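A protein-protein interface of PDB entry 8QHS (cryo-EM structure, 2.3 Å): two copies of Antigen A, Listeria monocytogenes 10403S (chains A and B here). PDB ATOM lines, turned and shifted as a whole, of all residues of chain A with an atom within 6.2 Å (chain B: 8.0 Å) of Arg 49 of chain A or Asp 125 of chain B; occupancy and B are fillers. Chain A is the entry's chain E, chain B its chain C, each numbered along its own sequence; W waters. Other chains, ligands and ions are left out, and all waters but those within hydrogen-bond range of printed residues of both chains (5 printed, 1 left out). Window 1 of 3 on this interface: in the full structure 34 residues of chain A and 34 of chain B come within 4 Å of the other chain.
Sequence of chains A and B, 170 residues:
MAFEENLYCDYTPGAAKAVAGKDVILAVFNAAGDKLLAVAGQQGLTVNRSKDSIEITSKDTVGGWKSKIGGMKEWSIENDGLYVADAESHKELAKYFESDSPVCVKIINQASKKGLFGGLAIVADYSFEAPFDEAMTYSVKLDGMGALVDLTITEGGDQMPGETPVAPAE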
ATOM      1  N   VAL A  47      37.303 -13.057  24.960  1.00  0.00           N
ATOM      2  CA  VAL A  47      36.383 -12.996  23.834  1.00  0.00           C
ATOM      3  C   VAL A  47      36.154 -11.528  23.515  1.00  0.00           C
ATOM      4  O   VAL A  47      35.563 -10.802  24.318  1.00  0.00           O
ATOM      5  CB  VAL A  47      35.059 -13.714  24.137  1.00  0.00           C
ATOM      6  CG1 VAL A  47      34.157 -13.697  22.922  1.00  0.00           C
ATOM      7  CG2 VAL A  47      35.319 -15.132  24.590  1.00  0.00           C
ATOM      8  N   ASN A  48      36.626 -11.091  22.356  1.00  0.00           N
ATOM      9  CA  ASN A  48      36.491  -9.709  21.915  1.00  0.00           C
ATOM     10  C   ASN A  48      35.362  -9.620  20.902  1.00  0.00           C
ATOM     11  O   ASN A  48      35.361 -10.351  19.913  1.00  0.00           O
ATOM     12  CB  ASN A  48      37.788  -9.198  21.292  1.00  0.00           C
ATOM     13  CG  ASN A  48      38.951  -9.262  22.240  1.00  0.00           C
ATOM     14  OD1 ASN A  48      38.986  -8.555  23.239  1.00  0.00           O
ATOM     15  ND2 ASN A  48      39.919 -10.112  21.931  1.00  0.00           N
ATOM     16  N   ARG A  49      34.402  -8.739  21.155  1.00  0.00           N
ATOM     17  CA  ARG A  49      33.368  -8.405  20.184  1.00  0.00           C
ATOM     18  C   ARG A  49      33.254  -6.895  20.102  1.00  0.00           C
ATOM     19  O   ARG A  49      33.035  -6.234  21.118  1.00  0.00           O
ATOM     20  CB  ARG A  49      32.013  -8.998  20.558  1.00  0.00           C
ATOM     21  CG  ARG A  49      31.940 -10.489  20.517  1.00  0.00           C
ATOM     22  CD  ARG A  49      31.276 -11.006  21.756  1.00  0.00           C
ATOM     23  NE  ARG A  49      29.860 -11.260  21.550  1.00  0.00           N
ATOM     24  CZ  ARG A  49      28.891 -10.814  22.336  1.00  0.00           C
ATOM     25  NH1 ARG A  49      29.167 -10.074  23.394  1.00  0.00           N
ATOM     26  NH2 ARG A  49      27.637 -11.114  22.056  1.00  0.00           N
ATOM     27  N   SER A  50      33.394  -6.353  18.902  1.00  0.00           N
ATOM     28  CA  SER A  50      33.331  -4.917  18.710  1.00  0.00           C
ATOM     29  C   SER A  50      32.465  -4.603  17.503  1.00  0.00           C
ATOM     30  O   SER A  50      32.248  -5.445  16.633  1.00  0.00           O
ATOM     31  CB  SER A  50      34.728  -4.308  18.542  1.00  0.00           C
ATOM     32  OG  SER A  50      35.397  -4.841  17.418  1.00  0.00           O
ATOM     33  N   LYS A  51      31.965  -3.377  17.472  1.00  0.00           N
ATOM     34  CA  LYS A  51      31.145  -2.868  16.386  1.00  0.00           C
ATOM     35  C   LYS A  51      31.696  -1.515  15.969  1.00  0.00           C
ATOM     36  O   LYS A  51      32.116  -0.729  16.821  1.00  0.00           O
ATOM     37  CB  LYS A  51      29.680  -2.747  16.819  1.00  0.00           C
ATOM     38  CG  LYS A  51      28.747  -2.262  15.737  1.00  0.00           C
ATOM     39  CD  LYS A  51      27.319  -2.170  16.231  1.00  0.00           C
ATOM     40  CE  LYS A  51      26.892  -3.459  16.890  1.00  0.00           C
ATOM     41  NZ  LYS A  51      25.437  -3.517  17.146  1.00  0.00           N
ATOM     42  N   GLU A  74      32.794  -7.396  14.418  1.00  0.00           N
ATOM     43  CA  GLU A  74      33.894  -8.333  14.277  1.00  0.00           C
ATOM     44  C   GLU A  74      34.196  -8.929  15.639  1.00  0.00           C
ATOM     45  O   GLU A  74      33.828  -8.371  16.672  1.00  0.00           O
ATOM     46  CB  GLU A  74      35.144  -7.663  13.693  1.00  0.00           C
ATOM     47  CG  GLU A  74      35.718  -6.568  14.549  1.00  0.00           C
ATOM     48  CD  GLU A  74      36.898  -5.880  13.903  1.00  0.00           C
ATOM     49  OE1 GLU A  74      37.062  -5.991  12.673  1.00  0.00           O
ATOM     50  OE2 GLU A  74      37.674  -5.227  14.628  1.00  0.00           O
ATOM     51  N   TRP A  75      34.851 -10.081  15.642  1.00  0.00           N
ATOM     52  CA  TRP A  75      35.186 -10.738  16.891  1.00  0.00           C
ATOM     53  C   TRP A  75      36.520 -11.452  16.770  1.00  0.00           C
ATOM     54  O   TRP A  75      36.975 -11.776  15.674  1.00  0.00           O
ATOM     55  CB  TRP A  75      34.098 -11.729  17.328  1.00  0.00           C
ATOM     56  CG  TRP A  75      33.902 -12.906  16.426  1.00  0.00           C
ATOM     57  CD1 TRP A  75      33.181 -12.942  15.278  1.00  0.00           C
ATOM     58  CD2 TRP A  75      34.413 -14.227  16.619  1.00  0.00           C
ATOM     59  NE1 TRP A  75      33.216 -14.192  14.735  1.00  0.00           N
ATOM     60  CE2 TRP A  75      33.962 -15.006  15.542  1.00  0.00           C
ATOM     61  CE3 TRP A  75      35.211 -14.825  17.596  1.00  0.00           C
ATOM     62  CZ2 TRP A  75      34.285 -16.353  15.409  1.00  0.00           C
ATOM     63  CZ3 TRP A  75      35.530 -16.155  17.462  1.00  0.00           C
ATOM     64  CH2 TRP A  75      35.068 -16.908  16.377  1.00  0.00           C
ATOM     65  N   SER A  76      37.145 -11.678  17.916  1.00  0.00           N
ATOM     66  CA  SER A  76      38.311 -12.536  18.008  1.00  0.00           C
ATOM     67  C   SER A  76      38.319 -13.195  19.375  1.00  0.00           C
ATOM     68  O   SER A  76      37.659 -12.735  20.306  1.00  0.00           O
ATOM     69  CB  SER A  76      39.622 -11.773  17.779  1.00  0.00           C
ATOM     70  OG  SER A  76      39.736 -10.662  18.639  1.00  0.00           O
ATOM     71  N   PHE A 117      29.439 -19.033  23.261  1.00  0.00           N
ATOM     72  CA  PHE A 117      29.687 -18.465  21.946  1.00  0.00           C
ATOM     73  C   PHE A 117      30.238 -19.543  21.032  1.00  0.00           C
ATOM     74  O   PHE A 117      30.907 -20.469  21.488  1.00  0.00           O
ATOM     75  CB  PHE A 117      30.669 -17.290  22.014  1.00  0.00           C
ATOM     76  CG  PHE A 117      30.270 -16.234  22.987  1.00  0.00           C
ATOM     77  CD1 PHE A 117      29.292 -15.313  22.662  1.00  0.00           C
ATOM     78  CD2 PHE A 117      30.855 -16.172  24.236  1.00  0.00           C
ATOM     79  CE1 PHE A 117      28.913 -14.350  23.560  1.00  0.00           C
ATOM     80  CE2 PHE A 117      30.479 -15.212  25.134  1.00  0.00           C
ATOM     81  CZ  PHE A 117      29.505 -14.301  24.796  1.00  0.00           C
ATOM     82  N   LEU A 148      29.732 -14.467  15.149  1.00  0.00           N
ATOM     83  CA  LEU A 148      29.925 -15.194  16.391  1.00  0.00           C
ATOM     84  C   LEU A 148      28.555 -15.380  17.024  1.00  0.00           C
ATOM     85  O   LEU A 148      27.942 -14.409  17.474  1.00  0.00           O
ATOM     86  CB  LEU A 148      30.871 -14.454  17.334  1.00  0.00           C
ATOM     87  CG  LEU A 148      31.240 -15.205  18.612  1.00  0.00           C
ATOM     88  CD1 LEU A 148      32.017 -16.469  18.309  1.00  0.00           C
ATOM     89  CD2 LEU A 148      32.019 -14.311  19.546  1.00  0.00           C
ATOM     90  N   ASP A 150      25.846 -15.930  19.580  1.00  0.00           N
ATOM     91  CA  ASP A 150      25.659 -15.758  21.014  1.00  0.00           C
ATOM     92  C   ASP A 150      24.738 -16.872  21.495  1.00  0.00           C
ATOM     93  O   ASP A 150      23.527 -16.820  21.276  1.00  0.00           O
ATOM     94  CB  ASP A 150      25.075 -14.380  21.305  1.00  0.00           C
ATOM     95  CG  ASP A 150      25.283 -13.939  22.733  1.00  0.00           C
ATOM     96  OD1 ASP A 150      25.677 -12.777  22.939  1.00  0.00           O
ATOM     97  OD2 ASP A 150      25.039 -14.735  23.654  1.00  0.00           O
ATOM     98  N   ILE B  77      30.309   5.505  27.208  1.00  0.00           N
ATOM     99  CA  ILE B  77      30.263   4.941  28.548  1.00  0.00           C
ATOM    100  C   ILE B  77      30.987   3.608  28.521  1.00  0.00           C
ATOM    101  O   ILE B  77      30.730   2.772  27.650  1.00  0.00           O
ATOM    102  CB  ILE B  77      28.820   4.786  29.058  1.00  0.00           C
ATOM    103  CG1 ILE B  77      28.283   6.136  29.530  1.00  0.00           C
ATOM    104  CG2 ILE B  77      28.755   3.782  30.193  1.00  0.00           C
ATOM    105  CD1 ILE B  77      26.806   6.165  29.739  1.00  0.00           C
ATOM    106  N   GLU B  78      31.901   3.422  29.458  1.00  0.00           N
ATOM    107  CA  GLU B  78      32.600   2.162  29.632  1.00  0.00           C
ATOM    108  C   GLU B  78      32.173   1.546  30.952  1.00  0.00           C
ATOM    109  O   GLU B  78      32.165   2.221  31.983  1.00  0.00           O
ATOM    110  CB  GLU B  78      34.112   2.368  29.580  1.00  0.00           C
ATOM    111  CG  GLU B  78      34.636   2.446  28.166  1.00  0.00           C
ATOM    112  CD  GLU B  78      35.845   3.344  28.025  1.00  0.00           C
ATOM    113  OE1 GLU B  78      36.148   4.110  28.965  1.00  0.00           O
ATOM    114  OE2 GLU B  78      36.498   3.286  26.962  1.00  0.00           O
ATOM    115  N   ASN B  79      31.800   0.276  30.911  1.00  0.00           N
ATOM    116  CA  ASN B  79      31.320  -0.436  32.083  1.00  0.00           C
ATOM    117  C   ASN B  79      31.905  -1.837  32.086  1.00  0.00           C
ATOM    118  O   ASN B  79      31.864  -2.535  31.073  1.00  0.00           O
ATOM    119  CB  ASN B  79      29.791  -0.482  32.100  1.00  0.00           C
ATOM    120  CG  ASN B  79      29.237  -1.060  33.377  1.00  0.00           C
ATOM    121  OD1 ASN B  79      28.611  -2.108  33.369  1.00  0.00           O
ATOM    122  ND2 ASN B  79      29.466  -0.377  34.482  1.00  0.00           N
ATOM    123  N   TYR B  83      30.589 -11.042  35.005  1.00  0.00           N
ATOM    124  CA  TYR B  83      29.687 -11.476  33.952  1.00  0.00           C
ATOM    125  C   TYR B  83      28.903 -12.701  34.394  1.00  0.00           C
ATOM    126  O   TYR B  83      29.490 -13.717  34.770  1.00  0.00           O
ATOM    127  CB  TYR B  83      30.449 -11.796  32.669  1.00  0.00           C
ATOM    128  CG  TYR B  83      29.534 -12.198  31.544  1.00  0.00           C
ATOM    129  CD1 TYR B  83      28.469 -11.391  31.173  1.00  0.00           C
ATOM    130  CD2 TYR B  83      29.717 -13.390  30.867  1.00  0.00           C
ATOM    131  CE1 TYR B  83      27.632 -11.750  30.158  1.00  0.00           C
ATOM    132  CE2 TYR B  83      28.883 -13.759  29.844  1.00  0.00           C
ATOM    133  CZ  TYR B  83      27.842 -12.935  29.490  1.00  0.00           C
ATOM    134  OH  TYR B  83      27.006 -13.297  28.470  1.00  0.00           O
ATOM    135  N   HIS B  90      22.131  -8.602  31.010  1.00  0.00           N
ATOM    136  CA  HIS B  90      23.125  -9.063  30.051  1.00  0.00           C
ATOM    137  C   HIS B  90      22.470  -9.710  28.840  1.00  0.00           C
ATOM    138  O   HIS B  90      22.993  -9.623  27.727  1.00  0.00           O
ATOM    139  CB  HIS B  90      24.102 -10.016  30.728  1.00  0.00           C
ATOM    140  CG  HIS B  90      25.124  -9.315  31.561  1.00  0.00           C
ATOM    141  ND1 HIS B  90      26.080  -8.487  31.018  1.00  0.00           N
ATOM    142  CD2 HIS B  90      25.322  -9.292  32.899  1.00  0.00           C
ATOM    143  CE1 HIS B  90      26.835  -7.998  31.982  1.00  0.00           C
ATOM    144  NE2 HIS B  90      26.395  -8.471  33.133  1.00  0.00           N
ATOM    145  N   LEU B  93      21.530  -6.672  26.807  1.00  0.00           N
ATOM    146  CA  LEU B  93      22.712  -6.164  26.117  1.00  0.00           C
ATOM    147  C   LEU B  93      23.107  -7.067  24.962  1.00  0.00           C
ATOM    148  O   LEU B  93      23.514  -6.584  23.901  1.00  0.00           O
ATOM    149  CB  LEU B  93      23.874  -6.018  27.097  1.00  0.00           C
ATOM    150  CG  LEU B  93      23.845  -4.841  28.064  1.00  0.00           C
ATOM    151  CD1 LEU B  93      25.047  -4.881  28.976  1.00  0.00           C
ATOM    152  CD2 LEU B  93      23.779  -3.531  27.308  1.00  0.00           C
ATOM    153  N   ALA B  94      22.989  -8.383  25.149  1.00  0.00           N
ATOM    154  CA  ALA B  94      23.304  -9.322  24.079  1.00  0.00           C
ATOM    155  C   ALA B  94      22.375  -9.137  22.888  1.00  0.00           C
ATOM    156  O   ALA B  94      22.823  -9.159  21.738  1.00  0.00           O
ATOM    157  CB  ALA B  94      23.229 -10.754  24.601  1.00  0.00           C
ATOM    158  N   LYS B  95      21.079  -8.951  23.143  1.00  0.00           N
ATOM    159  CA  LYS B  95      20.137  -8.748  22.047  1.00  0.00           C
ATOM    160  C   LYS B  95      20.368  -7.411  21.358  1.00  0.00           C
ATOM    161  O   LYS B  95      20.211  -7.305  20.139  1.00  0.00           O
ATOM    162  CB  LYS B  95      18.703  -8.846  22.557  1.00  0.00           C
ATOM    163  CG  LYS B  95      18.290 -10.237  22.955  1.00  0.00           C
ATOM    164  CD  LYS B  95      17.031 -10.214  23.781  1.00  0.00           C
ATOM    165  CE  LYS B  95      17.049 -11.298  24.833  1.00  0.00           C
ATOM    166  NZ  LYS B  95      16.650 -10.764  26.161  1.00  0.00           N
ATOM    167  N   PHE B  97      23.291  -5.933  21.058  1.00  0.00           N
ATOM    168  CA  PHE B  97      24.490  -6.113  20.253  1.00  0.00           C
ATOM    169  C   PHE B  97      24.205  -6.954  19.015  1.00  0.00           C
ATOM    170  O   PHE B  97      24.756  -6.695  17.942  1.00  0.00           O
ATOM    171  CB  PHE B  97      25.593  -6.745  21.105  1.00  0.00           C
ATOM    172  CG  PHE B  97      26.924  -6.796  20.429  1.00  0.00           C
ATOM    173  CD1 PHE B  97      27.653  -5.641  20.219  1.00  0.00           C
ATOM    174  CD2 PHE B  97      27.446  -8.000  19.994  1.00  0.00           C
ATOM    175  CE1 PHE B  97      28.877  -5.686  19.596  1.00  0.00           C
ATOM    176  CE2 PHE B  97      28.666  -8.050  19.370  1.00  0.00           C
ATOM    177  CZ  PHE B  97      29.384  -6.890  19.170  1.00  0.00           C
ATOM    178  N   GLU B  98      23.328  -7.950  19.139  1.00  0.00           N
ATOM    179  CA  GLU B  98      23.041  -8.837  18.016  1.00  0.00           C
ATOM    180  C   GLU B  98      22.163  -8.157  16.977  1.00  0.00           C
ATOM    181  O   GLU B  98      22.365  -8.336  15.773  1.00  0.00           O
ATOM    182  CB  GLU B  98      22.368 -10.112  18.520  1.00  0.00           C
ATOM    183  CG  GLU B  98      22.170 -11.251  17.505  1.00  0.00           C
ATOM    184  CD  GLU B  98      23.356 -11.493  16.567  1.00  0.00           C
ATOM    185  OE1 GLU B  98      23.576 -10.713  15.618  1.00  0.00           O
ATOM    186  OE2 GLU B  98      24.089 -12.479  16.787  1.00  0.00           O
ATOM    187  N   ILE B 122      25.154   3.187  20.848  1.00  0.00           N
ATOM    188  CA  ILE B 122      25.518   1.938  20.199  1.00  0.00           C
ATOM    189  C   ILE B 122      26.260   1.065  21.198  1.00  0.00           C
ATOM    190  O   ILE B 122      27.115   1.544  21.949  1.00  0.00           O
ATOM    191  CB  ILE B 122      26.394   2.207  18.961  1.00  0.00           C
ATOM    192  CG1 ILE B 122      25.653   3.070  17.944  1.00  0.00           C
ATOM    193  CG2 ILE B 122      26.867   0.914  18.330  1.00  0.00           C
ATOM    194  CD1 ILE B 122      26.511   4.146  17.343  1.00  0.00           C
ATOM    195  N   VAL B 123      25.938  -0.225  21.219  1.00  0.00           N
ATOM    196  CA  VAL B 123      26.786  -1.182  21.921  1.00  0.00           C
ATOM    197  C   VAL B 123      27.999  -1.393  21.029  1.00  0.00           C
ATOM    198  O   VAL B 123      27.976  -2.185  20.086  1.00  0.00           O
ATOM    199  CB  VAL B 123      26.064  -2.503  22.234  1.00  0.00           C
ATOM    200  CG1 VAL B 123      26.949  -3.387  23.086  1.00  0.00           C
ATOM    201  CG2 VAL B 123      24.748  -2.246  22.932  1.00  0.00           C
ATOM    202  N   ALA B 124      29.070  -0.659  21.317  1.00  0.00           N
ATOM    203  CA  ALA B 124      30.211  -0.628  20.411  1.00  0.00           C
ATOM    204  C   ALA B 124      31.186  -1.753  20.714  1.00  0.00           C
ATOM    205  O   ALA B 124      31.929  -2.198  19.836  1.00  0.00           O
ATOM    206  CB  ALA B 124      30.905   0.727  20.500  1.00  0.00           C
ATOM    207  N   ASP B 125      31.201  -2.224  21.952  1.00  0.00           N
ATOM    208  CA  ASP B 125      32.092  -3.289  22.370  1.00  0.00           C
ATOM    209  C   ASP B 125      31.435  -4.042  23.511  1.00  0.00           C
ATOM    210  O   ASP B 125      30.873  -3.429  24.419  1.00  0.00           O
ATOM    211  CB  ASP B 125      33.448  -2.732  22.798  1.00  0.00           C
ATOM    212  CG  ASP B 125      34.479  -3.807  22.990  1.00  0.00           C
ATOM    213  OD1 ASP B 125      35.254  -4.063  22.050  1.00  0.00           O
ATOM    214  OD2 ASP B 125      34.516  -4.403  24.085  1.00  0.00           O
ATOM    215  N   TYR B 126      31.489  -5.366  23.454  1.00  0.00           N
ATOM    216  CA  TYR B 126      30.901  -6.221  24.475  1.00  0.00           C
ATOM    217  C   TYR B 126      31.754  -7.474  24.573  1.00  0.00           C
ATOM    218  O   TYR B 126      31.532  -8.437  23.839  1.00  0.00           O
ATOM    219  CB  TYR B 126      29.445  -6.547  24.130  1.00  0.00           C
ATOM    220  CG  TYR B 126      28.622  -7.083  25.271  1.00  0.00           C
ATOM    221  CD1 TYR B 126      29.096  -7.060  26.570  1.00  0.00           C
ATOM    222  CD2 TYR B 126      27.366  -7.619  25.044  1.00  0.00           C
ATOM    223  CE1 TYR B 126      28.346  -7.556  27.606  1.00  0.00           C
ATOM    224  CE2 TYR B 126      26.611  -8.115  26.072  1.00  0.00           C
ATOM    225  CZ  TYR B 126      27.105  -8.079  27.350  1.00  0.00           C
ATOM    226  OH  TYR B 126      26.352  -8.574  28.377  1.00  0.00           O
ATOM    227  N   SER B 127      32.722  -7.459  25.483  1.00  0.00           N
ATOM    228  CA  SER B 127      33.779  -8.456  25.513  1.00  0.00           C
ATOM    229  C   SER B 127      33.845  -9.098  26.887  1.00  0.00           C
ATOM    230  O   SER B 127      33.253  -8.614  27.847  1.00  0.00           O
ATOM    231  CB  SER B 127      35.134  -7.844  25.148  1.00  0.00           C
ATOM    232  OG  SER B 127      35.095  -7.222  23.883  1.00  0.00           O
ATOM    233  N   PHE B 128      34.576 -10.205  26.965  1.00  0.00           N
ATOM    234  CA  PHE B 128      34.615 -11.039  28.156  1.00  0.00           C
ATOM    235  C   PHE B 128      36.018 -11.571  28.392  1.00  0.00           C
ATOM    236  O   PHE B 128      36.765 -11.825  27.447  1.00  0.00           O
ATOM    237  CB  PHE B 128      33.624 -12.201  28.034  1.00  0.00           C
ATOM    238  CG  PHE B 128      32.268 -11.773  27.578  1.00  0.00           C
ATOM    239  CD1 PHE B 128      31.349 -11.275  28.476  1.00  0.00           C
ATOM    240  CD2 PHE B 128      31.926 -11.826  26.241  1.00  0.00           C
ATOM    241  CE1 PHE B 128      30.115 -10.857  28.053  1.00  0.00           C
ATOM    242  CE2 PHE B 128      30.697 -11.409  25.820  1.00  0.00           C
ATOM    243  CZ  PHE B 128      29.785 -10.928  26.728  1.00  0.00           C
ATOM    244  N   TYR B 138      32.959  -9.163  32.257  1.00  0.00           N
ATOM    245  CA  TYR B 138      32.530  -8.572  31.005  1.00  0.00           C
ATOM    246  C   TYR B 138      33.094  -7.164  30.917  1.00  0.00           C
ATOM    247  O   TYR B 138      33.502  -6.582  31.921  1.00  0.00           O
ATOM    248  CB  TYR B 138      31.000  -8.536  30.890  1.00  0.00           C
ATOM    249  CG  TYR B 138      30.360  -7.504  31.778  1.00  0.00           C
ATOM    250  CD1 TYR B 138      30.123  -6.214  31.323  1.00  0.00           C
ATOM    251  CD2 TYR B 138      30.005  -7.813  33.078  1.00  0.00           C
ATOM    252  CE1 TYR B 138      29.559  -5.277  32.136  1.00  0.00           C
ATOM    253  CE2 TYR B 138      29.434  -6.882  33.891  1.00  0.00           C
ATOM    254  CZ  TYR B 138      29.215  -5.616  33.417  1.00  0.00           C
ATOM    255  OH  TYR B 138      28.644  -4.684  34.228  1.00  0.00           O
ATOM    256  N   SER B 139      33.112  -6.629  29.709  1.00  0.00           N
ATOM    257  CA  SER B 139      33.451  -5.241  29.457  1.00  0.00           C
ATOM    258  C   SER B 139      32.565  -4.761  28.324  1.00  0.00           C
ATOM    259  O   SER B 139      32.493  -5.407  27.277  1.00  0.00           O
ATOM    260  CB  SER B 139      34.929  -5.096  29.102  1.00  0.00           C
ATOM    261  OG  SER B 139      35.241  -3.772  28.737  1.00  0.00           O
ATOM    262  N   VAL B 140      31.874  -3.651  28.534  1.00  0.00           N
ATOM    263  CA  VAL B 140      30.967  -3.114  27.533  1.00  0.00           C
ATOM    264  C   VAL B 140      31.330  -1.660  27.279  1.00  0.00           C
ATOM    265  O   VAL B 140      31.676  -0.924  28.209  1.00  0.00           O
ATOM    266  CB  VAL B 140      29.490  -3.276  27.949  1.00  0.00           C
ATOM    267  CG1 VAL B 140      29.159  -2.451  29.169  1.00  0.00           C
ATOM    268  CG2 VAL B 140      28.573  -2.928  26.802  1.00  0.00           C
ATOM    269  N   LYS B 141      31.301  -1.265  26.016  1.00  0.00           N
ATOM    270  CA  LYS B 141      31.485   0.118  25.616  1.00  0.00           C
ATOM    271  C   LYS B 141      30.224   0.598  24.919  1.00  0.00           C
ATOM    272  O   LYS B 141      29.751  -0.038  23.976  1.00  0.00           O
ATOM    273  CB  LYS B 141      32.694   0.278  24.698  1.00  0.00           C
ATOM    274  CG  LYS B 141      32.916   1.701  24.259  1.00  0.00           C
ATOM    275  CD  LYS B 141      34.241   1.884  23.570  1.00  0.00           C
ATOM    276  CE  LYS B 141      34.480   3.349  23.252  1.00  0.00           C
ATOM    277  NZ  LYS B 141      33.381   3.904  22.416  1.00  0.00           N
ATOM    278  N   LEU B 142      29.681   1.711  25.390  1.00  0.00           N
ATOM    279  CA  LEU B 142      28.477   2.299  24.829  1.00  0.00           C
ATOM    280  C   LEU B 142      28.834   3.602  24.134  1.00  0.00           C
ATOM    281  O   LEU B 142      29.162   4.589  24.792  1.00  0.00           O
ATOM    282  CB  LEU B 142      27.432   2.528  25.919  1.00  0.00           C
ATOM    283  CG  LEU B 142      26.994   1.232  26.596  1.00  0.00           C
ATOM    284  CD1 LEU B 142      26.193   1.504  27.847  1.00  0.00           C
ATOM    285  CD2 LEU B 142      26.216   0.373  25.624  1.00  0.00           C
ATOM    286  N   ASP B 143      28.771   3.600  22.811  1.00  0.00           N
ATOM    287  CA  ASP B 143      29.104   4.758  21.997  1.00  0.00           C
ATOM    288  C   ASP B 143      27.861   5.609  21.794  1.00  0.00           C
ATOM    289  O   ASP B 143      26.856   5.126  21.270  1.00  0.00           O
ATOM    290  CB  ASP B 143      29.672   4.324  20.647  1.00  0.00           C
ATOM    291  CG  ASP B 143      30.848   5.160  20.214  1.00  0.00           C
ATOM    292  OD1 ASP B 143      30.782   6.400  20.349  1.00  0.00           O
ATOM    293  OD2 ASP B 143      31.844   4.583  19.739  1.00  0.00           O
HETATM  294  O   HOH W   1      23.703 -14.675  17.979  1.00  0.00           O
HETATM  295  O   HOH W   2      23.884  -1.226  19.236  1.00  0.00           O
HETATM  296  O   HOH W   3      25.073 -10.947  21.183  1.00  0.00           O
HETATM  297  O   HOH W   4      34.237  -0.951  19.153  1.00  0.00           O
HETATM  298  O   HOH W   5      32.698   2.077  17.931  1.00  0.00           O
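The backbone carbonyl oxygen (O) of Phe 97 of chain B lies within hydrogen-bond range of the side-chain amino group (NZ) of Lys 51 of chain A (3.3 Å). The backbone NH of Lys 51 of chain A lies within hydrogen-bond range of the backbone carbonyl oxygen of Ala 124 of chain B, at 2.6 Å. NH1 of Arg 49 of chain A is in hydrogen-bond range of O of Tyr 126 of chain B, 2.9 Å away. OG of Ser 127 of chain B sits at hydrogen-bond distance from N of Arg 49 of chain A. N of Val 47 of chain A sits at hydrogen-bond distance from O of Phe 128 of chain B (2.8 Å). OD1 of Asp 125 of chain B sits close to O of Arg 49 of chain A (3.2 Å).
The backbone NH of Ala 124 of chain B lies within hydrogen-bond range of the backbone carbonyl oxygen of Lys 141 of chain B (2.8 Å). The side-chain carboxylate (OD2) of Asp 125 of chain B sits at hydrogen-bond distance from the side-chain hydroxyl (OG) of Ser 127 of chain B, at 2.9 Å. The backbone NH (N) of Lys 141 of chain B is in hydrogen-bond range of the backbone carbonyl oxygen (O) of Asp 125 of chain B (2.7 Å). N of Ser 139 of chain B lies within hydrogen-bond range of O of Ser 127 of chain B, 2.7 Å away.
Asn 48 of chain A touches Ser 127 of chain B (CA to OG, 3.5 Å). CB of Arg 49 of chain A touches CZ of Phe 97 of chain B, at 3.6 Å. CE2 of Phe 128 of chain B touches NH1 of Arg 49 of chain A, 3.2 Å away. Ala 124 of chain B touches Ser 50 of chain A (O to CA, 3.3 Å). CB of Ser 50 of chain A touches OD1 of Asp 125 of chain B (3.6 Å). Ile 122 of chain B touches Lys 51 of chain A (CG2 to CD, 3.8 Å). Lys 51 of chain A touches Val 123 of chain B. Phe 117 of chain A touches Phe 128 of chain B. OD1 of Asp 150 of chain A touches CB of Ala 94 of chain B (3.6 Å).
Of chain B, only Phe 97, Asp 125, Tyr 126, Ser 127 and Phe 128 come within 4 Å of Arg 49 of chain A. Of chain A, only Arg 49 and Ser 50 come within 4 Å of Asp 125 of chain B. Of the printed residues of chain A, Ala 124 of chain B touches Ser 50 (3.3 Å) and Lys 51 (2.6 Å). Of the printed residues of chain A, Tyr 126 of chain B touches Arg 49. Printed residues of chain B within 4 Å of Ser 50 of chain A: Ala 124 and Asp 125. Printed residues of chain A within 4 Å of Val 123 of chain B: Lys 51 (3.6 Å). Printed residues of chain B within 4 Å of Asn 48 of chain A: Ser 127 (3.5 Å). Tyr 138 of chain B touches none of the printed residues of chain A. The nearest printed residue of chain A that does not touch Ala 124 of chain B is Arg 49 of chain A (4.4 Å).
Of the 23 printed residues of chain B, 9 touch a printed residue of chain A. Hydrophobic or aromatic side chains of chain B that line the printed part of chain A: Ala 94, Phe 97, Ile 122, Tyr 126 and Phe 128. Among the printed residues, 16 pairs touch across the chains. Among the printed residues, no Asp or Glu carboxylate lies within 4 Å of a Lys or Arg side-chain nitrogen of the other chain.
No position is printed for both chains. Of the 16 pairs that touch across the chains among the printed residues, none has its exchanged pair printed and touching as well.
Water W1 bridges OE2 of Glu 98 of chain B (2.5 Å) and N of Asp 150 of chain A (3.0 Å). Water W4 lies within hydrogen-bond range of O of Ala 124 of chain B (2.7 Å) and O of Lys 51 of chain A (3.2 Å). Water W2 bridges N of Val 123 of chain B (3.0 Å) and NZ of Lys 51 of chain A (3.5 Å). Water W5 bridges O of Lys 51 of chain A (3.1 Å) and OD2 of Asp 143 of chain B (3.2 Å).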
